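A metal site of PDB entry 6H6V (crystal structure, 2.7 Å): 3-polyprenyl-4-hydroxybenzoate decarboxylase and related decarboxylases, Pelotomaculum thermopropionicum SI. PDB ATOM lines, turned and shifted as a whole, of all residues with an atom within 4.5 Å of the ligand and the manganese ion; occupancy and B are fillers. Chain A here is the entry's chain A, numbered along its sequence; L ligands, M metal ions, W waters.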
ATOM      1  N   THR A 132     -17.620  13.923 -15.202  1.00  0.00           N
ATOM      2  CA  THR A 132     -16.590  13.553 -16.168  1.00  0.00           C
ATOM      3  C   THR A 132     -16.534  14.415 -17.413  1.00  0.00           C
ATOM      4  O   THR A 132     -15.527  14.377 -18.128  1.00  0.00           O
ATOM      5  CB  THR A 132     -16.768  12.090 -16.616  1.00  0.00           C
ATOM      6  OG1 THR A 132     -18.094  11.875 -17.134  1.00  0.00           O
ATOM      7  CG2 THR A 132     -16.502  11.150 -15.467  1.00  0.00           C
ATOM      8  N   ASN A 147      -8.647  30.310 -19.683  1.00  0.00           N
ATOM      9  CA  ASN A 147      -8.234  28.974 -20.078  1.00  0.00           C
ATOM     10  C   ASN A 147      -9.436  28.049 -19.918  1.00  0.00           C
ATOM     11  O   ASN A 147     -10.308  28.292 -19.108  1.00  0.00           O
ATOM     12  CB  ASN A 147      -7.083  28.496 -19.196  1.00  0.00           C
ATOM     13  CG  ASN A 147      -6.445  27.206 -19.703  1.00  0.00           C
ATOM     14  OD1 ASN A 147      -5.598  27.210 -20.575  1.00  0.00           O
ATOM     15  ND2 ASN A 147      -6.840  26.101 -19.108  1.00  0.00           N
ATOM     16  N   VAL A 148      -9.453  26.995 -20.728  1.00  0.00           N
ATOM     17  CA  VAL A 148     -10.432  25.933 -20.637  1.00  0.00           C
ATOM     18  C   VAL A 148      -9.697  24.595 -20.618  1.00  0.00           C
ATOM     19  O   VAL A 148      -8.773  24.389 -21.405  1.00  0.00           O
ATOM     20  CB  VAL A 148     -11.424  25.953 -21.826  1.00  0.00           C
ATOM     21  CG1 VAL A 148     -12.589  25.008 -21.575  1.00  0.00           C
ATOM     22  CG2 VAL A 148     -11.943  27.348 -22.060  1.00  0.00           C
ATOM     23  N   SER A 149     -10.112  23.708 -19.729  1.00  0.00           N
ATOM     24  CA  SER A 149      -9.613  22.334 -19.663  1.00  0.00           C
ATOM     25  C   SER A 149     -10.687  21.476 -19.036  1.00  0.00           C
ATOM     26  O   SER A 149     -11.592  21.995 -18.430  1.00  0.00           O
ATOM     27  CB  SER A 149      -8.324  22.250 -18.835  1.00  0.00           C
ATOM     28  OG  SER A 149      -8.390  23.009 -17.628  1.00  0.00           O
ATOM     29  N   ILE A 150     -10.581  20.172 -19.169  1.00  0.00           N
ATOM     30  CA  ILE A 150     -11.513  19.229 -18.580  1.00  0.00           C
ATOM     31  C   ILE A 150     -10.821  18.503 -17.433  1.00  0.00           C
ATOM     32  O   ILE A 150      -9.692  18.062 -17.583  1.00  0.00           O
ATOM     33  CB  ILE A 150     -12.019  18.210 -19.604  1.00  0.00           C
ATOM     34  CG1 ILE A 150     -12.743  18.924 -20.756  1.00  0.00           C
ATOM     35  CG2 ILE A 150     -12.959  17.217 -18.928  1.00  0.00           C
ATOM     36  CD1 ILE A 150     -13.216  18.023 -21.876  1.00  0.00           C
ATOM     37  N   HIS A 151     -11.487  18.367 -16.295  1.00  0.00           N
ATOM     38  CA  HIS A 151     -10.930  17.737 -15.106  1.00  0.00           C
ATOM     39  C   HIS A 151     -11.970  16.898 -14.432  1.00  0.00           C
ATOM     40  O   HIS A 151     -13.130  17.323 -14.320  1.00  0.00           O
ATOM     41  CB  HIS A 151     -10.440  18.762 -14.110  1.00  0.00           C
ATOM     42  CG  HIS A 151      -9.439  19.709 -14.675  1.00  0.00           C
ATOM     43  ND1 HIS A 151      -8.083  19.549 -14.465  1.00  0.00           N
ATOM     44  CD2 HIS A 151      -9.584  20.785 -15.487  1.00  0.00           C
ATOM     45  CE1 HIS A 151      -7.441  20.512 -15.114  1.00  0.00           C
ATOM     46  NE2 HIS A 151      -8.336  21.267 -15.739  1.00  0.00           N
ATOM     47  N   ARG A 152     -11.576  15.713 -13.968  1.00  0.00           N
ATOM     48  CA  ARG A 152     -12.489  14.858 -13.232  1.00  0.00           C
ATOM     49  C   ARG A 152     -12.814  15.498 -11.875  1.00  0.00           C
ATOM     50  O   ARG A 152     -11.953  16.121 -11.239  1.00  0.00           O
ATOM     51  CB  ARG A 152     -11.896  13.456 -13.063  1.00  0.00           C
ATOM     52  CG  ARG A 152     -10.774  13.311 -12.052  1.00  0.00           C
ATOM     53  CD  ARG A 152     -10.310  11.880 -11.988  1.00  0.00           C
ATOM     54  NE  ARG A 152      -9.342  11.674 -10.926  1.00  0.00           N
ATOM     55  CZ  ARG A 152      -8.232  10.955 -11.018  1.00  0.00           C
ATOM     56  NH1 ARG A 152      -7.846  10.361 -12.155  1.00  0.00           N
ATOM     57  NH2 ARG A 152      -7.441  10.876  -9.961  1.00  0.00           N
ATOM     58  N   LEU A 164      -8.685  16.669  -9.806  1.00  0.00           N
ATOM     59  CA  LEU A 164      -7.320  16.355 -10.257  1.00  0.00           C
ATOM     60  C   LEU A 164      -6.872  17.458 -11.191  1.00  0.00           C
ATOM     61  O   LEU A 164      -7.476  17.669 -12.245  1.00  0.00           O
ATOM     62  CB  LEU A 164      -7.251  15.032 -10.991  1.00  0.00           C
ATOM     63  CG  LEU A 164      -5.890  14.645 -11.565  1.00  0.00           C
ATOM     64  CD1 LEU A 164      -4.925  14.294 -10.458  1.00  0.00           C
ATOM     65  CD2 LEU A 164      -6.012  13.519 -12.568  1.00  0.00           C
ATOM     66  N   ILE A 165      -5.811  18.161 -10.792  1.00  0.00           N
ATOM     67  CA  ILE A 165      -5.206  19.172 -11.643  1.00  0.00           C
ATOM     68  C   ILE A 165      -3.779  18.701 -11.961  1.00  0.00           C
ATOM     69  O   ILE A 165      -2.874  18.811 -11.124  1.00  0.00           O
ATOM     70  CB  ILE A 165      -5.191  20.565 -10.978  1.00  0.00           C
ATOM     71  CG1 ILE A 165      -6.538  20.874 -10.308  1.00  0.00           C
ATOM     72  CG2 ILE A 165      -4.859  21.637 -12.011  1.00  0.00           C
ATOM     73  CD1 ILE A 165      -6.637  22.270  -9.718  1.00  0.00           C
ATOM     74  N   LEU A 166      -3.586  18.180 -13.181  1.00  0.00           N
ATOM     75  CA  LEU A 166      -2.247  17.909 -13.690  1.00  0.00           C
ATOM     76  C   LEU A 166      -1.548  19.230 -13.984  1.00  0.00           C
ATOM     77  O   LEU A 166      -2.217  20.261 -14.190  1.00  0.00           O
ATOM     78  CB  LEU A 166      -2.302  17.031 -14.955  1.00  0.00           C
ATOM     79  CG  LEU A 166      -2.918  15.633 -14.810  1.00  0.00           C
ATOM     80  CD1 LEU A 166      -3.240  15.029 -16.165  1.00  0.00           C
ATOM     81  CD2 LEU A 166      -2.019  14.698 -14.032  1.00  0.00           C
ATOM     82  N   ARG A 168      -0.483  21.754 -15.886  1.00  0.00           N
ATOM     83  CA  ARG A 168      -0.513  22.517 -17.142  1.00  0.00           C
ATOM     84  C   ARG A 168      -1.115  23.889 -16.777  1.00  0.00           C
ATOM     85  O   ARG A 168      -0.698  24.456 -15.794  1.00  0.00           O
ATOM     86  CB  ARG A 168      -1.258  21.791 -18.286  1.00  0.00           C
ATOM     87  CG  ARG A 168      -0.485  20.670 -18.982  1.00  0.00           C
ATOM     88  CD  ARG A 168      -0.669  19.325 -18.261  1.00  0.00           C
ATOM     89  NE  ARG A 168      -1.905  18.629 -18.665  1.00  0.00           N
ATOM     90  CZ  ARG A 168      -2.001  17.423 -19.248  1.00  0.00           C
ATOM     91  NH1 ARG A 168      -0.925  16.682 -19.512  1.00  0.00           N
ATOM     92  NH2 ARG A 168      -3.198  16.957 -19.522  1.00  0.00           N
ATOM     93  N   HIS A 169      -2.082  24.425 -17.542  1.00  0.00           N
ATOM     94  CA  HIS A 169      -2.450  25.829 -17.403  1.00  0.00           C
ATOM     95  C   HIS A 169      -3.304  26.117 -16.173  1.00  0.00           C
ATOM     96  O   HIS A 169      -3.129  27.148 -15.527  1.00  0.00           O
ATOM     97  CB  HIS A 169      -3.157  26.338 -18.660  1.00  0.00           C
ATOM     98  CG  HIS A 169      -2.274  26.371 -19.874  1.00  0.00           C
ATOM     99  ND1 HIS A 169      -2.768  26.428 -21.157  1.00  0.00           N
ATOM    100  CD2 HIS A 169      -0.920  26.352 -19.988  1.00  0.00           C
ATOM    101  CE1 HIS A 169      -1.762  26.451 -22.014  1.00  0.00           C
ATOM    102  NE2 HIS A 169      -0.632  26.404 -21.331  1.00  0.00           N
ATOM    103  N   LEU A 170      -4.249  25.246 -15.837  1.00  0.00           N
ATOM    104  CA  LEU A 170      -5.047  25.486 -14.651  1.00  0.00           C
ATOM    105  C   LEU A 170      -4.163  25.482 -13.408  1.00  0.00           C
ATOM    106  O   LEU A 170      -4.378  26.266 -12.506  1.00  0.00           O
ATOM    107  CB  LEU A 170      -6.189  24.483 -14.495  1.00  0.00           C
ATOM    108  CG  LEU A 170      -7.153  24.776 -13.331  1.00  0.00           C
ATOM    109  CD1 LEU A 170      -7.787  26.165 -13.444  1.00  0.00           C
ATOM    110  CD2 LEU A 170      -8.225  23.692 -13.272  1.00  0.00           C
ATOM    111  N   SER A 200     -11.284  22.394 -25.764  1.00  0.00           N
ATOM    112  CA  SER A 200     -10.728  22.391 -24.411  1.00  0.00           C
ATOM    113  C   SER A 200      -9.452  21.557 -24.338  1.00  0.00           C
ATOM    114  O   SER A 200      -8.609  21.814 -23.483  1.00  0.00           O
ATOM    115  CB  SER A 200     -11.721  21.855 -23.383  1.00  0.00           C
ATOM    116  OG  SER A 200     -11.949  20.462 -23.592  1.00  0.00           O
ATOM    117  N   GLN A 201      -9.324  20.585 -25.237  1.00  0.00           N
ATOM    118  CA  GLN A 201      -8.120  19.752 -25.349  1.00  0.00           C
ATOM    119  C   GLN A 201      -7.027  20.314 -26.235  1.00  0.00           C
ATOM    120  O   GLN A 201      -5.970  19.711 -26.339  1.00  0.00           O
ATOM    121  CB  GLN A 201      -8.484  18.389 -25.914  1.00  0.00           C
ATOM    122  CG  GLN A 201      -9.525  17.672 -25.072  1.00  0.00           C
ATOM    123  CD  GLN A 201      -9.067  17.539 -23.659  1.00  0.00           C
ATOM    124  OE1 GLN A 201      -9.612  18.199 -22.778  1.00  0.00           O
ATOM    125  NE2 GLN A 201      -8.083  16.715 -23.450  1.00  0.00           N
ATOM    126  N   ALA A 202      -7.269  21.429 -26.915  1.00  0.00           N
ATOM    127  CA  ALA A 202      -6.235  22.031 -27.753  1.00  0.00           C
ATOM    128  C   ALA A 202      -5.071  22.417 -26.874  1.00  0.00           C
ATOM    129  O   ALA A 202      -5.232  22.906 -25.737  1.00  0.00           O
ATOM    130  CB  ALA A 202      -6.753  23.236 -28.508  1.00  0.00           C
ATOM    131  N   THR A 204      -1.652  24.446 -26.504  1.00  0.00           N
ATOM    132  CA  THR A 204      -1.216  25.744 -27.061  1.00  0.00           C
ATOM    133  C   THR A 204      -0.270  26.512 -26.155  1.00  0.00           C
ATOM    134  O   THR A 204      -0.007  26.129 -25.012  1.00  0.00           O
ATOM    135  CB  THR A 204      -2.416  26.700 -27.305  1.00  0.00           C
ATOM    136  OG1 THR A 204      -2.935  27.181 -26.054  1.00  0.00           O
ATOM    137  CG2 THR A 204      -3.534  26.000 -28.066  1.00  0.00           C
ATOM    138  N   VAL A 208      -3.518  31.636 -24.794  1.00  0.00           N
ATOM    139  CA  VAL A 208      -4.664  31.543 -25.723  1.00  0.00           C
ATOM    140  C   VAL A 208      -5.926  30.903 -25.124  1.00  0.00           C
ATOM    141  O   VAL A 208      -5.884  29.877 -24.451  1.00  0.00           O
ATOM    142  CB  VAL A 208      -4.338  31.021 -27.160  1.00  0.00           C
ATOM    143  CG1 VAL A 208      -2.840  30.912 -27.391  1.00  0.00           C
ATOM    144  CG2 VAL A 208      -5.058  29.731 -27.523  1.00  0.00           C
ATOM    145  N   GLU A 210      -9.198  28.931 -25.247  1.00  0.00           N
ATOM    146  CA  GLU A 210      -9.765  27.805 -25.986  1.00  0.00           C
ATOM    147  C   GLU A 210     -11.226  27.991 -26.384  1.00  0.00           C
ATOM    148  O   GLU A 210     -11.693  27.344 -27.333  1.00  0.00           O
ATOM    149  CB  GLU A 210      -9.612  26.510 -25.191  1.00  0.00           C
ATOM    150  CG  GLU A 210      -8.150  26.065 -25.113  1.00  0.00           C
ATOM    151  CD  GLU A 210      -7.453  26.475 -23.798  1.00  0.00           C
ATOM    152  OE1 GLU A 210      -7.941  27.398 -23.111  1.00  0.00           O
ATOM    153  OE2 GLU A 210      -6.418  25.862 -23.459  1.00  0.00           O
ATOM    154  N   ILE A 289     -19.184  11.467 -19.772  1.00  0.00           N
ATOM    155  CA  ILE A 289     -18.213  10.757 -20.599  1.00  0.00           C
ATOM    156  C   ILE A 289     -17.765   9.545 -19.778  1.00  0.00           C
ATOM    157  O   ILE A 289     -17.220   9.692 -18.669  1.00  0.00           O
ATOM    158  CB  ILE A 289     -17.007  11.639 -20.963  1.00  0.00           C
ATOM    159  CG1 ILE A 289     -17.431  12.776 -21.886  1.00  0.00           C
ATOM    160  CG2 ILE A 289     -15.947  10.816 -21.693  1.00  0.00           C
ATOM    161  CD1 ILE A 289     -16.377  13.861 -22.107  1.00  0.00           C
ATOM    162  N   HIS A 296     -14.135   9.615 -24.794  1.00  0.00           N
ATOM    163  CA  HIS A 296     -13.028  10.016 -23.940  1.00  0.00           C
ATOM    164  C   HIS A 296     -11.712  10.026 -24.681  1.00  0.00           C
ATOM    165  O   HIS A 296     -10.964  11.000 -24.633  1.00  0.00           O
ATOM    166  CB  HIS A 296     -12.913   9.072 -22.723  1.00  0.00           C
ATOM    167  CG  HIS A 296     -11.907   9.492 -21.706  1.00  0.00           C
ATOM    168  ND1 HIS A 296     -11.656   8.755 -20.577  1.00  0.00           N
ATOM    169  CD2 HIS A 296     -11.081  10.564 -21.631  1.00  0.00           C
ATOM    170  CE1 HIS A 296     -10.722   9.342 -19.850  1.00  0.00           C
ATOM    171  NE2 HIS A 296     -10.380  10.464 -20.460  1.00  0.00           N
ATOM    172  N   LEU A 299     -11.277  12.614 -27.808  1.00  0.00           N
ATOM    173  CA  LEU A 299     -11.198  14.035 -27.463  1.00  0.00           C
ATOM    174  C   LEU A 299      -9.740  14.459 -27.371  1.00  0.00           C
ATOM    175  O   LEU A 299      -9.310  15.409 -28.025  1.00  0.00           O
ATOM    176  CB  LEU A 299     -11.908  14.370 -26.152  1.00  0.00           C
ATOM    177  CG  LEU A 299     -13.407  14.591 -26.227  1.00  0.00           C
ATOM    178  CD1 LEU A 299     -13.988  14.747 -24.839  1.00  0.00           C
ATOM    179  CD2 LEU A 299     -13.763  15.786 -27.072  1.00  0.00           C
ATOM    180  N   GLY A 300      -8.979  13.732 -26.548  1.00  0.00           N
ATOM    181  CA  GLY A 300      -7.542  13.938 -26.450  1.00  0.00           C
ATOM    182  C   GLY A 300      -6.787  13.465 -27.683  1.00  0.00           C
ATOM    183  O   GLY A 300      -5.808  14.082 -28.083  1.00  0.00           O
HETATM  184  N1  LIG L   1      -6.543  16.782 -16.956  1.00  0.00           N
HETATM  185  C1  LIG L   1      -6.287  16.847 -15.627  1.00  0.00           C
HETATM  186  O1  LIG L   1      -5.299  17.504 -15.216  1.00  0.00           O
HETATM  187  N2  LIG L   1      -7.054  16.209 -14.736  1.00  0.00           N
HETATM  188  C2  LIG L   1      -8.119  15.508 -15.112  1.00  0.00           C
HETATM  189  O2  LIG L   1      -8.816  14.959 -14.245  1.00  0.00           O
HETATM  190  C3  LIG L   1      -8.466  15.397 -16.545  1.00  0.00           C
HETATM  191  N3  LIG L   1      -9.523  14.714 -16.975  1.00  0.00           N
HETATM  192  C4  LIG L   1      -9.824  14.672 -18.302  1.00  0.00           C
HETATM  193  C5  LIG L   1     -10.946  13.987 -18.748  1.00  0.00           C
HETATM  194  C6  LIG L   1     -11.284  13.930 -20.088  1.00  0.00           C
HETATM  195  C7  LIG L   1     -12.522  13.167 -20.482  1.00  0.00           C
HETATM  196  C8  LIG L   1     -10.464  14.618 -21.119  1.00  0.00           C
HETATM  197  C9  LIG L   1     -10.815  14.521 -22.601  1.00  0.00           C
HETATM  198  C10 LIG L   1      -9.346  15.301 -20.682  1.00  0.00           C
HETATM  199  C11 LIG L   1      -8.988  15.366 -19.330  1.00  0.00           C
HETATM  200  N4  LIG L   1      -7.852  16.083 -18.855  1.00  0.00           N
HETATM  201  C12 LIG L   1      -7.595  16.104 -17.468  1.00  0.00           C
HETATM  202  C13 LIG L   1      -6.884  16.721 -19.755  1.00  0.00           C
HETATM  203  C14 LIG L   1      -6.904  18.194 -19.903  1.00  0.00           C
HETATM  204  O3  LIG L   1      -8.284  18.592 -19.879  1.00  0.00           O
HETATM  205  C15 LIG L   1      -6.189  18.489 -21.211  1.00  0.00           C
HETATM  206  O4  LIG L   1      -4.882  17.929 -21.190  1.00  0.00           O
HETATM  207  C16 LIG L   1      -6.159  19.966 -21.451  1.00  0.00           C
HETATM  208  O5  LIG L   1      -5.878  20.211 -22.848  1.00  0.00           O
HETATM  209  C17 LIG L   1      -5.167  20.728 -20.586  1.00  0.00           C
HETATM  210  O6  LIG L   1      -5.355  22.081 -21.009  1.00  0.00           O
HETATM  211  P1  LIG L   1      -4.342  23.276 -20.588  1.00  0.00           P
HETATM  212  O7  LIG L   1      -4.093  23.059 -19.104  1.00  0.00           O
HETATM  213  O8  LIG L   1      -3.100  23.110 -21.436  1.00  0.00           O
HETATM  214  O9  LIG L   1      -5.059  24.571 -20.988  1.00  0.00           O
HETATM  215 MN    MN M   1      -4.586  26.333 -22.277  1.00  0.00          MN
HETATM  216  O   HOH W   1      -5.141  22.343 -17.013  1.00  0.00           O
HETATM  217  O   HOH W   2      -3.880  24.565 -23.623  1.00  0.00           O
HETATM  218  O   HOH W   3      -4.502  19.387 -17.001  1.00  0.00           O
HETATM  219  O   HOH W   4     -11.605  12.024 -16.343  1.00  0.00           O
HETATM  220  O   HOH W   5      -0.200  22.665 -21.379  1.00  0.00           O
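OE1 of Gln 201 lies within hydrogen-bond range of OG of Ser 200.
OE1 of Glu 210 lies within hydrogen-bond range of N of Val 148 (2.9 Å).
The backbone carbonyl oxygen (O) of Leu 164 sits at hydrogen-bond distance from a ring nitrogen (ND1) of His 151 (3.0 Å).
A ring nitrogen (NE2) of His 151 lies within hydrogen-bond range of the side-chain hydroxyl (OG) of Ser 149 (2.6 Å).
Residues that only touch the ligand: Val 148 (3.7 Å), Ser 149 (3.7 Å), His 151 (3.4 Å), Ile 165 (3.8 Å), Leu 170 (3.9 Å), His 296 (3.2 Å) and Leu 299 (3.7 Å).
Hydrophobic or aromatic side chains that line the ligand: Ile 150, His 151, Leu 164, Leu 166, His 169, His 296 and Leu 299.
The manganese ion is bound by ND1 of His 169, at 2.1 Å.
The manganese ion is bound by OD1 of Asn 147 (2.2 Å).
OE2 of Glu 210 binds the manganese ion (2.2 Å).
O9 of the ligand binds the manganese ion (2.2 Å).
Water W2 is bound to the manganese ion, at 2.3 Å.
An oxygen (O3) of the ligand is in hydrogen-bond range of the backbone NH of Ile 150 (2.9 Å).
The side-chain amide oxygen of Gln 201 is in hydrogen-bond range of an oxygen (O3) of the ligand, at 3.2 Å.
O of Leu 164 is in hydrogen-bond range of N2 of the ligand (2.9 Å).
N of His 169 sits at hydrogen-bond distance from O7 of the ligand, 2.9 Å away.
O2 of the ligand lies within hydrogen-bond range of N of Arg 152, at 2.9 Å.
O of Ile 150 is in hydrogen-bond range of O3 of the ligand (2.7 Å).
The backbone NH (N) of Leu 166 is in hydrogen-bond range of an oxygen (O1) of the ligand (2.7 Å).
NH2 of Arg 168 sits at hydrogen-bond distance from O4 of the ligand, at 2.6 Å.
O of Ser 200 is in hydrogen-bond range of O5 of the ligand (3.2 Å).
Three residues have an atom within 4 Å of the manganese ion: Asn 147, His 169 and Glu 210.
Water W2 bridges O8 of the ligand (2.7 Å) and O of Ala 202 (3.0 Å).
Water W1 lies within hydrogen-bond range of an oxygen (O7) of the ligand (2.4 Å), the backbone NH of Leu 170 (3.3 Å) and the side-chain hydroxyl of Ser 149 (3.4 Å).
Water W3 bridges an oxygen (O1) of the ligand (2.7 Å) and the guanidinium group of Arg 168 (3.2 Å).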
